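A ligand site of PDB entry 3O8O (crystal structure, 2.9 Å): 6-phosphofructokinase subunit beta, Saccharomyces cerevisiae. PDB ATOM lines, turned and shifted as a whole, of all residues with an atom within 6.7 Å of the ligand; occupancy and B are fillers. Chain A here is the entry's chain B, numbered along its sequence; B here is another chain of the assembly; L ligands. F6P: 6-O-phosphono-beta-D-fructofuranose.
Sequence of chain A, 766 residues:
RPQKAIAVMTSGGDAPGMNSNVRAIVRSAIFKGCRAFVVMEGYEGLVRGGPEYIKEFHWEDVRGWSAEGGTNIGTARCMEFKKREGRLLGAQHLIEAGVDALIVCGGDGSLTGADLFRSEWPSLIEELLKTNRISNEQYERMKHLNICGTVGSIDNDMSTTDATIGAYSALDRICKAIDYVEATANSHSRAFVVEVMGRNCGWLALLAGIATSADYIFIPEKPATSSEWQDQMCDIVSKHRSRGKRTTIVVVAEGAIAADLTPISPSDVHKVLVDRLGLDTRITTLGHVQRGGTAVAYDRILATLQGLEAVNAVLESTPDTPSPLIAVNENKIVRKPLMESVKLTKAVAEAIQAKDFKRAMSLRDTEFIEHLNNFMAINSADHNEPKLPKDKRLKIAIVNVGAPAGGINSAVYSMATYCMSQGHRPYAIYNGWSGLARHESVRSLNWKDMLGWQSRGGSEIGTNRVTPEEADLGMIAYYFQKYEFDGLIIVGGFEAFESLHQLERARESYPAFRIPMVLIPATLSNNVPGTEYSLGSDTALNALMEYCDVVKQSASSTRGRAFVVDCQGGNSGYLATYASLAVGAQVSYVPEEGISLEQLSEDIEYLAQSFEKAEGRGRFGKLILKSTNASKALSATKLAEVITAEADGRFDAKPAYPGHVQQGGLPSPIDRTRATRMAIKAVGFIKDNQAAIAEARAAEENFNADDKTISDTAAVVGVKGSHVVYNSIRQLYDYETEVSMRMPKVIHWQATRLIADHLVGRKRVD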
ATOM      1  N   GLY A  12      31.923 -21.446 -15.511  1.00  0.00           N
ATOM      2  CA  GLY A  12      31.536 -22.042 -14.255  1.00  0.00           C
ATOM      3  C   GLY A  12      31.093 -23.472 -14.451  1.00  0.00           C
ATOM      4  O   GLY A  12      31.281 -24.033 -15.539  1.00  0.00           O
ATOM      5  N   GLY A  13      30.510 -24.047 -13.405  1.00  0.00           N
ATOM      6  CA  GLY A  13      30.062 -25.427 -13.471  1.00  0.00           C
ATOM      7  C   GLY A  13      28.986 -25.573 -14.494  1.00  0.00           C
ATOM      8  O   GLY A  13      28.016 -24.807 -14.476  1.00  0.00           O
ATOM      9  N   ASP A  14      29.157 -26.520 -15.405  1.00  0.00           N
ATOM     10  CA  ASP A  14      28.182 -26.759 -16.467  1.00  0.00           C
ATOM     11  C   ASP A  14      26.894 -27.245 -15.836  1.00  0.00           C
ATOM     12  O   ASP A  14      26.908 -27.772 -14.719  1.00  0.00           O
ATOM     13  CB  ASP A  14      28.716 -27.813 -17.478  1.00  0.00           C
ATOM     14  CG  ASP A  14      28.838 -29.214 -16.865  1.00  0.00           C
ATOM     15  OD1 ASP A  14      29.110 -29.344 -15.649  1.00  0.00           O
ATOM     16  OD2 ASP A  14      28.674 -30.206 -17.601  1.00  0.00           O
ATOM     17  N   GLY A 152      22.972 -20.353 -15.242  1.00  0.00           N
ATOM     18  CA  GLY A 152      22.818 -21.782 -15.360  1.00  0.00           C
ATOM     19  C   GLY A 152      23.518 -22.446 -14.199  1.00  0.00           C
ATOM     20  O   GLY A 152      24.714 -22.264 -13.989  1.00  0.00           O
ATOM     21  N   SER A 153      22.768 -23.230 -13.448  1.00  0.00           N
ATOM     22  CA  SER A 153      23.320 -23.931 -12.296  1.00  0.00           C
ATOM     23  C   SER A 153      22.329 -24.935 -11.762  1.00  0.00           C
ATOM     24  O   SER A 153      21.129 -24.661 -11.728  1.00  0.00           O
ATOM     25  CB  SER A 153      23.676 -22.918 -11.208  1.00  0.00           C
ATOM     26  OG  SER A 153      24.240 -23.582 -10.109  1.00  0.00           O
ATOM     27  N   ILE A 154      22.803 -26.114 -11.355  1.00  0.00           N
ATOM     28  CA  ILE A 154      21.882 -27.105 -10.819  1.00  0.00           C
ATOM     29  C   ILE A 154      21.428 -26.793  -9.398  1.00  0.00           C
ATOM     30  O   ILE A 154      20.425 -27.368  -8.932  1.00  0.00           O
ATOM     31  CB  ILE A 154      22.479 -28.540 -10.800  1.00  0.00           C
ATOM     32  CG1 ILE A 154      23.776 -28.594 -10.004  1.00  0.00           C
ATOM     33  CG2 ILE A 154      22.709 -29.024 -12.197  1.00  0.00           C
ATOM     34  CD1 ILE A 154      24.279 -30.002  -9.802  1.00  0.00           C
ATOM     35  N   ASP A 155      22.147 -25.882  -8.718  1.00  0.00           N
ATOM     36  CA  ASP A 155      21.872 -25.492  -7.327  1.00  0.00           C
ATOM     37  C   ASP A 155      20.621 -24.652  -7.023  1.00  0.00           C
ATOM     38  O   ASP A 155      20.084 -24.744  -5.921  1.00  0.00           O
ATOM     39  CB  ASP A 155      23.082 -24.760  -6.755  1.00  0.00           C
ATOM     40  CG  ASP A 155      24.383 -25.548  -6.952  1.00  0.00           C
ATOM     41  OD1 ASP A 155      24.368 -26.799  -6.892  1.00  0.00           O
ATOM     42  OD2 ASP A 155      25.438 -24.892  -7.162  1.00  0.00           O
ATOM     43  N   ASP A 157      20.288 -21.409  -6.562  1.00  0.00           N
ATOM     44  CA  ASP A 157      20.558 -20.567  -5.413  1.00  0.00           C
ATOM     45  C   ASP A 157      20.867 -19.098  -5.752  1.00  0.00           C
ATOM     46  O   ASP A 157      21.558 -18.415  -4.999  1.00  0.00           O
ATOM     47  CB  ASP A 157      21.702 -21.143  -4.578  1.00  0.00           C
ATOM     48  CG  ASP A 157      23.026 -21.062  -5.296  1.00  0.00           C
ATOM     49  OD1 ASP A 157      23.127 -20.344  -6.313  1.00  0.00           O
ATOM     50  OD2 ASP A 157      23.980 -21.708  -4.832  1.00  0.00           O
ATOM     51  N   MET A 197      23.852 -32.843  -3.993  1.00  0.00           N
ATOM     52  CA  MET A 197      24.545 -31.596  -4.279  1.00  0.00           C
ATOM     53  C   MET A 197      23.727 -30.369  -3.944  1.00  0.00           C
ATOM     54  O   MET A 197      22.669 -30.476  -3.321  1.00  0.00           O
ATOM     55  CB  MET A 197      24.936 -31.509  -5.765  1.00  0.00           C
ATOM     56  CG  MET A 197      25.963 -32.519  -6.198  1.00  0.00           C
ATOM     57  SD  MET A 197      26.709 -31.990  -7.710  1.00  0.00           S
ATOM     58  CE  MET A 197      28.218 -32.933  -7.748  1.00  0.00           C
ATOM     59  N   GLY A 198      24.220 -29.211  -4.354  1.00  0.00           N
ATOM     60  CA  GLY A 198      23.524 -27.972  -4.096  1.00  0.00           C
ATOM     61  C   GLY A 198      24.399 -26.907  -3.463  1.00  0.00           C
ATOM     62  O   GLY A 198      23.952 -25.786  -3.210  1.00  0.00           O
ATOM     63  N   ARG A 199      25.656 -27.256  -3.221  1.00  0.00           N
ATOM     64  CA  ARG A 199      26.579 -26.301  -2.614  1.00  0.00           C
ATOM     65  C   ARG A 199      26.019 -25.846  -1.265  1.00  0.00           C
ATOM     66  O   ARG A 199      25.939 -26.627  -0.318  1.00  0.00           O
ATOM     67  CB  ARG A 199      26.751 -25.103  -3.541  1.00  0.00           C
ATOM     68  CG  ARG A 199      27.850 -24.168  -3.165  1.00  0.00           C
ATOM     69  CD  ARG A 199      28.001 -23.064  -4.220  1.00  0.00           C
ATOM     70  NE  ARG A 199      28.447 -23.556  -5.526  1.00  0.00           N
ATOM     71  CZ  ARG A 199      29.708 -23.853  -5.827  1.00  0.00           C
ATOM     72  NH1 ARG A 199      30.658 -23.701  -4.913  1.00  0.00           N
ATOM     73  NH2 ARG A 199      30.052 -24.301  -7.025  1.00  0.00           N
ATOM     74  N   ASN A 200      25.593 -24.581  -1.195  1.00  0.00           N
ATOM     75  CA  ASN A 200      25.070 -24.065   0.068  1.00  0.00           C
ATOM     76  C   ASN A 200      23.572 -23.892   0.056  1.00  0.00           C
ATOM     77  O   ASN A 200      23.000 -23.340   0.997  1.00  0.00           O
ATOM     78  CB  ASN A 200      25.730 -22.720   0.404  1.00  0.00           C
ATOM     79  CG  ASN A 200      27.252 -22.839   0.610  1.00  0.00           C
ATOM     80  OD1 ASN A 200      27.714 -23.634   1.435  1.00  0.00           O
ATOM     81  ND2 ASN A 200      28.018 -22.051  -0.138  1.00  0.00           N
ATOM     82  N   LEU A 204      17.530 -28.520  -3.860  1.00  0.00           N
ATOM     83  CA  LEU A 204      17.568 -29.880  -4.387  1.00  0.00           C
ATOM     84  C   LEU A 204      17.209 -30.927  -3.352  1.00  0.00           C
ATOM     85  O   LEU A 204      16.416 -31.842  -3.637  1.00  0.00           O
ATOM     86  CB  LEU A 204      18.944 -30.192  -4.958  1.00  0.00           C
ATOM     87  CG  LEU A 204      19.258 -29.581  -6.325  1.00  0.00           C
ATOM     88  CD1 LEU A 204      20.723 -29.837  -6.666  1.00  0.00           C
ATOM     89  CD2 LEU A 204      18.347 -30.169  -7.392  1.00  0.00           C
ATOM     90  N   GLU A 254      24.425 -31.490   0.607  1.00  0.00           N
ATOM     91  CA  GLU A 254      25.857 -31.549   0.838  1.00  0.00           C
ATOM     92  C   GLU A 254      26.344 -30.468   1.819  1.00  0.00           C
ATOM     93  O   GLU A 254      27.240 -30.709   2.620  1.00  0.00           O
ATOM     94  CB  GLU A 254      26.627 -31.483  -0.498  1.00  0.00           C
ATOM     95  CG  GLU A 254      26.647 -30.140  -1.160  1.00  0.00           C
ATOM     96  CD  GLU A 254      27.363 -30.172  -2.487  1.00  0.00           C
ATOM     97  OE1 GLU A 254      28.182 -31.101  -2.734  1.00  0.00           O
ATOM     98  OE2 GLU A 254      27.097 -29.232  -3.278  1.00  0.00           O
ATOM     99  N   HIS A 288      28.466 -36.091  -9.231  1.00  0.00           N
ATOM    100  CA  HIS A 288      28.171 -35.468 -10.514  1.00  0.00           C
ATOM    101  C   HIS A 288      27.097 -36.047 -11.454  1.00  0.00           C
ATOM    102  O   HIS A 288      26.761 -35.389 -12.436  1.00  0.00           O
ATOM    103  CB  HIS A 288      29.471 -35.279 -11.295  1.00  0.00           C
ATOM    104  CG  HIS A 288      30.464 -34.420 -10.591  1.00  0.00           C
ATOM    105  ND1 HIS A 288      31.208 -34.880  -9.520  1.00  0.00           N
ATOM    106  CD2 HIS A 288      30.789 -33.114 -10.750  1.00  0.00           C
ATOM    107  CE1 HIS A 288      31.965 -33.891  -9.070  1.00  0.00           C
ATOM    108  NE2 HIS A 288      31.719 -32.816  -9.792  1.00  0.00           N
ATOM    109  N   ARG A 291      24.965 -33.626 -12.348  1.00  0.00           N
ATOM    110  CA  ARG A 291      25.372 -32.600 -13.293  1.00  0.00           C
ATOM    111  C   ARG A 291      25.214 -33.042 -14.739  1.00  0.00           C
ATOM    112  O   ARG A 291      25.119 -32.213 -15.643  1.00  0.00           O
ATOM    113  CB  ARG A 291      26.830 -32.216 -13.027  1.00  0.00           C
ATOM    114  CG  ARG A 291      27.018 -31.428 -11.761  1.00  0.00           C
ATOM    115  CD  ARG A 291      26.740 -29.951 -11.991  1.00  0.00           C
ATOM    116  NE  ARG A 291      27.840 -29.337 -12.723  1.00  0.00           N
ATOM    117  CZ  ARG A 291      29.052 -29.192 -12.210  1.00  0.00           C
ATOM    118  NH1 ARG A 291      29.299 -29.598 -10.964  1.00  0.00           N
ATOM    119  NH2 ARG A 291      30.022 -28.654 -12.944  1.00  0.00           N
ATOM    120  N   THR B 185      28.981 -33.931 -18.281  1.00  0.00           N
ATOM    121  CA  THR B 185      29.689 -32.966 -17.468  1.00  0.00           C
ATOM    122  C   THR B 185      31.199 -33.126 -17.594  1.00  0.00           C
ATOM    123  O   THR B 185      31.903 -32.131 -17.703  1.00  0.00           O
ATOM    124  CB  THR B 185      29.249 -33.059 -16.003  1.00  0.00           C
ATOM    125  OG1 THR B 185      29.826 -31.972 -15.261  1.00  0.00           O
ATOM    126  CG2 THR B 185      29.670 -34.399 -15.407  1.00  0.00           C
ATOM    127  N   HIS B 189      34.138 -30.017 -18.749  1.00  0.00           N
ATOM    128  CA  HIS B 189      35.314 -29.578 -18.021  1.00  0.00           C
ATOM    129  C   HIS B 189      36.562 -30.364 -18.382  1.00  0.00           C
ATOM    130  O   HIS B 189      37.557 -30.342 -17.653  1.00  0.00           O
ATOM    131  CB  HIS B 189      35.046 -29.682 -16.511  1.00  0.00           C
ATOM    132  CG  HIS B 189      33.896 -28.839 -16.023  1.00  0.00           C
ATOM    133  ND1 HIS B 189      33.952 -27.456 -15.990  1.00  0.00           N
ATOM    134  CD2 HIS B 189      32.678 -29.169 -15.533  1.00  0.00           C
ATOM    135  CE1 HIS B 189      32.818 -26.984 -15.505  1.00  0.00           C
ATOM    136  NE2 HIS B 189      32.023 -28.002 -15.222  1.00  0.00           N
ATOM    137  N   ARG B 191      37.564 -33.121 -17.892  1.00  0.00           N
ATOM    138  CA  ARG B 191      38.096 -33.820 -16.731  1.00  0.00           C
ATOM    139  C   ARG B 191      38.338 -35.304 -16.912  1.00  0.00           C
ATOM    140  O   ARG B 191      38.281 -35.834 -18.013  1.00  0.00           O
ATOM    141  CB  ARG B 191      37.147 -33.669 -15.571  1.00  0.00           C
ATOM    142  CG  ARG B 191      36.978 -32.252 -15.177  1.00  0.00           C
ATOM    143  CD  ARG B 191      35.920 -32.126 -14.131  1.00  0.00           C
ATOM    144  NE  ARG B 191      36.064 -30.863 -13.438  1.00  0.00           N
ATOM    145  CZ  ARG B 191      35.162 -30.373 -12.619  1.00  0.00           C
ATOM    146  NH1 ARG B 191      34.050 -31.054 -12.393  1.00  0.00           N
ATOM    147  NH2 ARG B 191      35.368 -29.219 -12.012  1.00  0.00           N
ATOM    148  N   PHE B 193      37.180 -38.849 -14.821  1.00  0.00           N
ATOM    149  CA  PHE B 193      36.454 -39.399 -13.680  1.00  0.00           C
ATOM    150  C   PHE B 193      36.810 -40.833 -13.410  1.00  0.00           C
ATOM    151  O   PHE B 193      36.965 -41.660 -14.322  1.00  0.00           O
ATOM    152  CB  PHE B 193      34.969 -39.337 -13.865  1.00  0.00           C
ATOM    153  CG  PHE B 193      34.391 -38.030 -13.533  1.00  0.00           C
ATOM    154  CD1 PHE B 193      34.713 -36.901 -14.293  1.00  0.00           C
ATOM    155  CD2 PHE B 193      33.419 -37.935 -12.534  1.00  0.00           C
ATOM    156  CE1 PHE B 193      34.046 -35.673 -14.069  1.00  0.00           C
ATOM    157  CE2 PHE B 193      32.739 -36.728 -12.282  1.00  0.00           C
ATOM    158  CZ  PHE B 193      33.049 -35.578 -13.070  1.00  0.00           C
ATOM    159  N   ASP B 280      42.332 -32.579 -13.991  1.00  0.00           N
ATOM    160  CA  ASP B 280      41.274 -32.233 -13.048  1.00  0.00           C
ATOM    161  C   ASP B 280      40.561 -33.570 -12.834  1.00  0.00           C
ATOM    162  O   ASP B 280      39.887 -34.053 -13.740  1.00  0.00           O
ATOM    163  CB  ASP B 280      40.310 -31.259 -13.705  1.00  0.00           C
ATOM    164  CG  ASP B 280      39.342 -30.630 -12.702  1.00  0.00           C
ATOM    165  OD1 ASP B 280      39.111 -31.235 -11.624  1.00  0.00           O
ATOM    166  OD2 ASP B 280      38.818 -29.539 -13.016  1.00  0.00           O
ATOM    167  N   LYS B 282      37.955 -36.358 -10.621  1.00  0.00           N
ATOM    168  CA  LYS B 282      36.912 -36.587  -9.634  1.00  0.00           C
ATOM    169  C   LYS B 282      36.647 -38.076  -9.457  1.00  0.00           C
ATOM    170  O   LYS B 282      36.990 -38.886 -10.322  1.00  0.00           O
ATOM    171  CB  LYS B 282      35.612 -35.886 -10.035  1.00  0.00           C
HETATM  172  O1  F6P L   1      28.273 -25.404  -9.436  1.00  0.00           O
HETATM  173  C1  F6P L   1      27.833 -25.855  -8.154  1.00  0.00           C
HETATM  174  C2  F6P L   1      28.181 -27.337  -7.988  1.00  0.00           C
HETATM  175  O2  F6P L   1      27.544 -28.145  -8.975  1.00  0.00           O
HETATM  176  C3  F6P L   1      27.778 -27.872  -6.618  1.00  0.00           C
HETATM  177  O3  F6P L   1      26.438 -28.393  -6.609  1.00  0.00           O
HETATM  178  C4  F6P L   1      28.906 -28.919  -6.358  1.00  0.00           C
HETATM  179  O4  F6P L   1      29.087 -29.184  -4.961  1.00  0.00           O
HETATM  180  C5  F6P L   1      30.125 -28.221  -7.039  1.00  0.00           C
HETATM  181  O5  F6P L   1      29.557 -27.535  -8.149  1.00  0.00           O
HETATM  182  C6  F6P L   1      31.108 -29.181  -7.653  1.00  0.00           C
HETATM  183  O6  F6P L   1      32.131 -28.371  -8.221  1.00  0.00           O
HETATM  184  P   F6P L   1      33.196 -29.289  -8.995  1.00  0.00           P
HETATM  185  O1P F6P L   1      32.502 -29.972 -10.119  1.00  0.00           O
HETATM  186  O2P F6P L   1      34.366 -28.366  -9.604  1.00  0.00           O
HETATM  187  O3P F6P L   1      33.824 -30.422  -8.002  1.00  0.00           O
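OE2 of Glu 254 is in hydrogen-bond range of O4 of the ligand, 2.6 Å away.
The side-chain carboxylate of Asp 155 lies within hydrogen-bond range of an oxygen (O3) of the ligand, at 2.6 Å.
An oxygen (O2P) of the ligand is in salt-bridge range of the guanidinium group (NH2) of Arg 191 of chain B (2.7 Å).
NH2 of Arg 199 sits close to O1 of the ligand.
An oxygen (O1P) of the ligand is in hydrogen-bond range of a ring nitrogen (NE2) of His 288 (3.0 Å).
NH1 of Arg 291 lies within salt-bridge range of O1P of the ligand (3.3 Å).
An oxygen (O3) of the ligand is in hydrogen-bond range of the backbone NH (N) of Gly 198 (3.3 Å).
An oxygen (O3) of the ligand sits close to the side-chain sulfur (SD) of Met 197 (3.8 Å).
OE2 of Glu 254 lies within hydrogen-bond range of N of Arg 199 (2.4 Å).
OE2 of Glu 254 lies within hydrogen-bond range of N of Gly 198 (3.1 Å).
NE of Arg 199 is in salt-bridge range of OD2 of Asp 155 (3.7 Å).
N of Asp 155 lies close to OG of Ser 153, 3.4 Å away.
The guanidinium group (NE) of Arg 191 of chain B is in salt-bridge range of the side-chain carboxylate (OD2) of Asp 280 of chain B, 3.1 Å away.
A ring nitrogen (NE2) of His 189 of chain B is in hydrogen-bond range of the guanidinium group (NH2) of Arg 291 (3.1 Å).
NH2 of Arg 291 is in salt-bridge range of OD1 of Asp 14.
Ile 154 touches the ligand (CD1 to O2, 3.8 Å).
Hydrophobic or aromatic side chains that line the ligand: Ile 154, Met 197 and His 288.
Of the 22 residues printed, 9 come within 4 Å of the ligand.
The nearest printed residue that does not touch the ligand is Gly 13 (4.4 Å).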
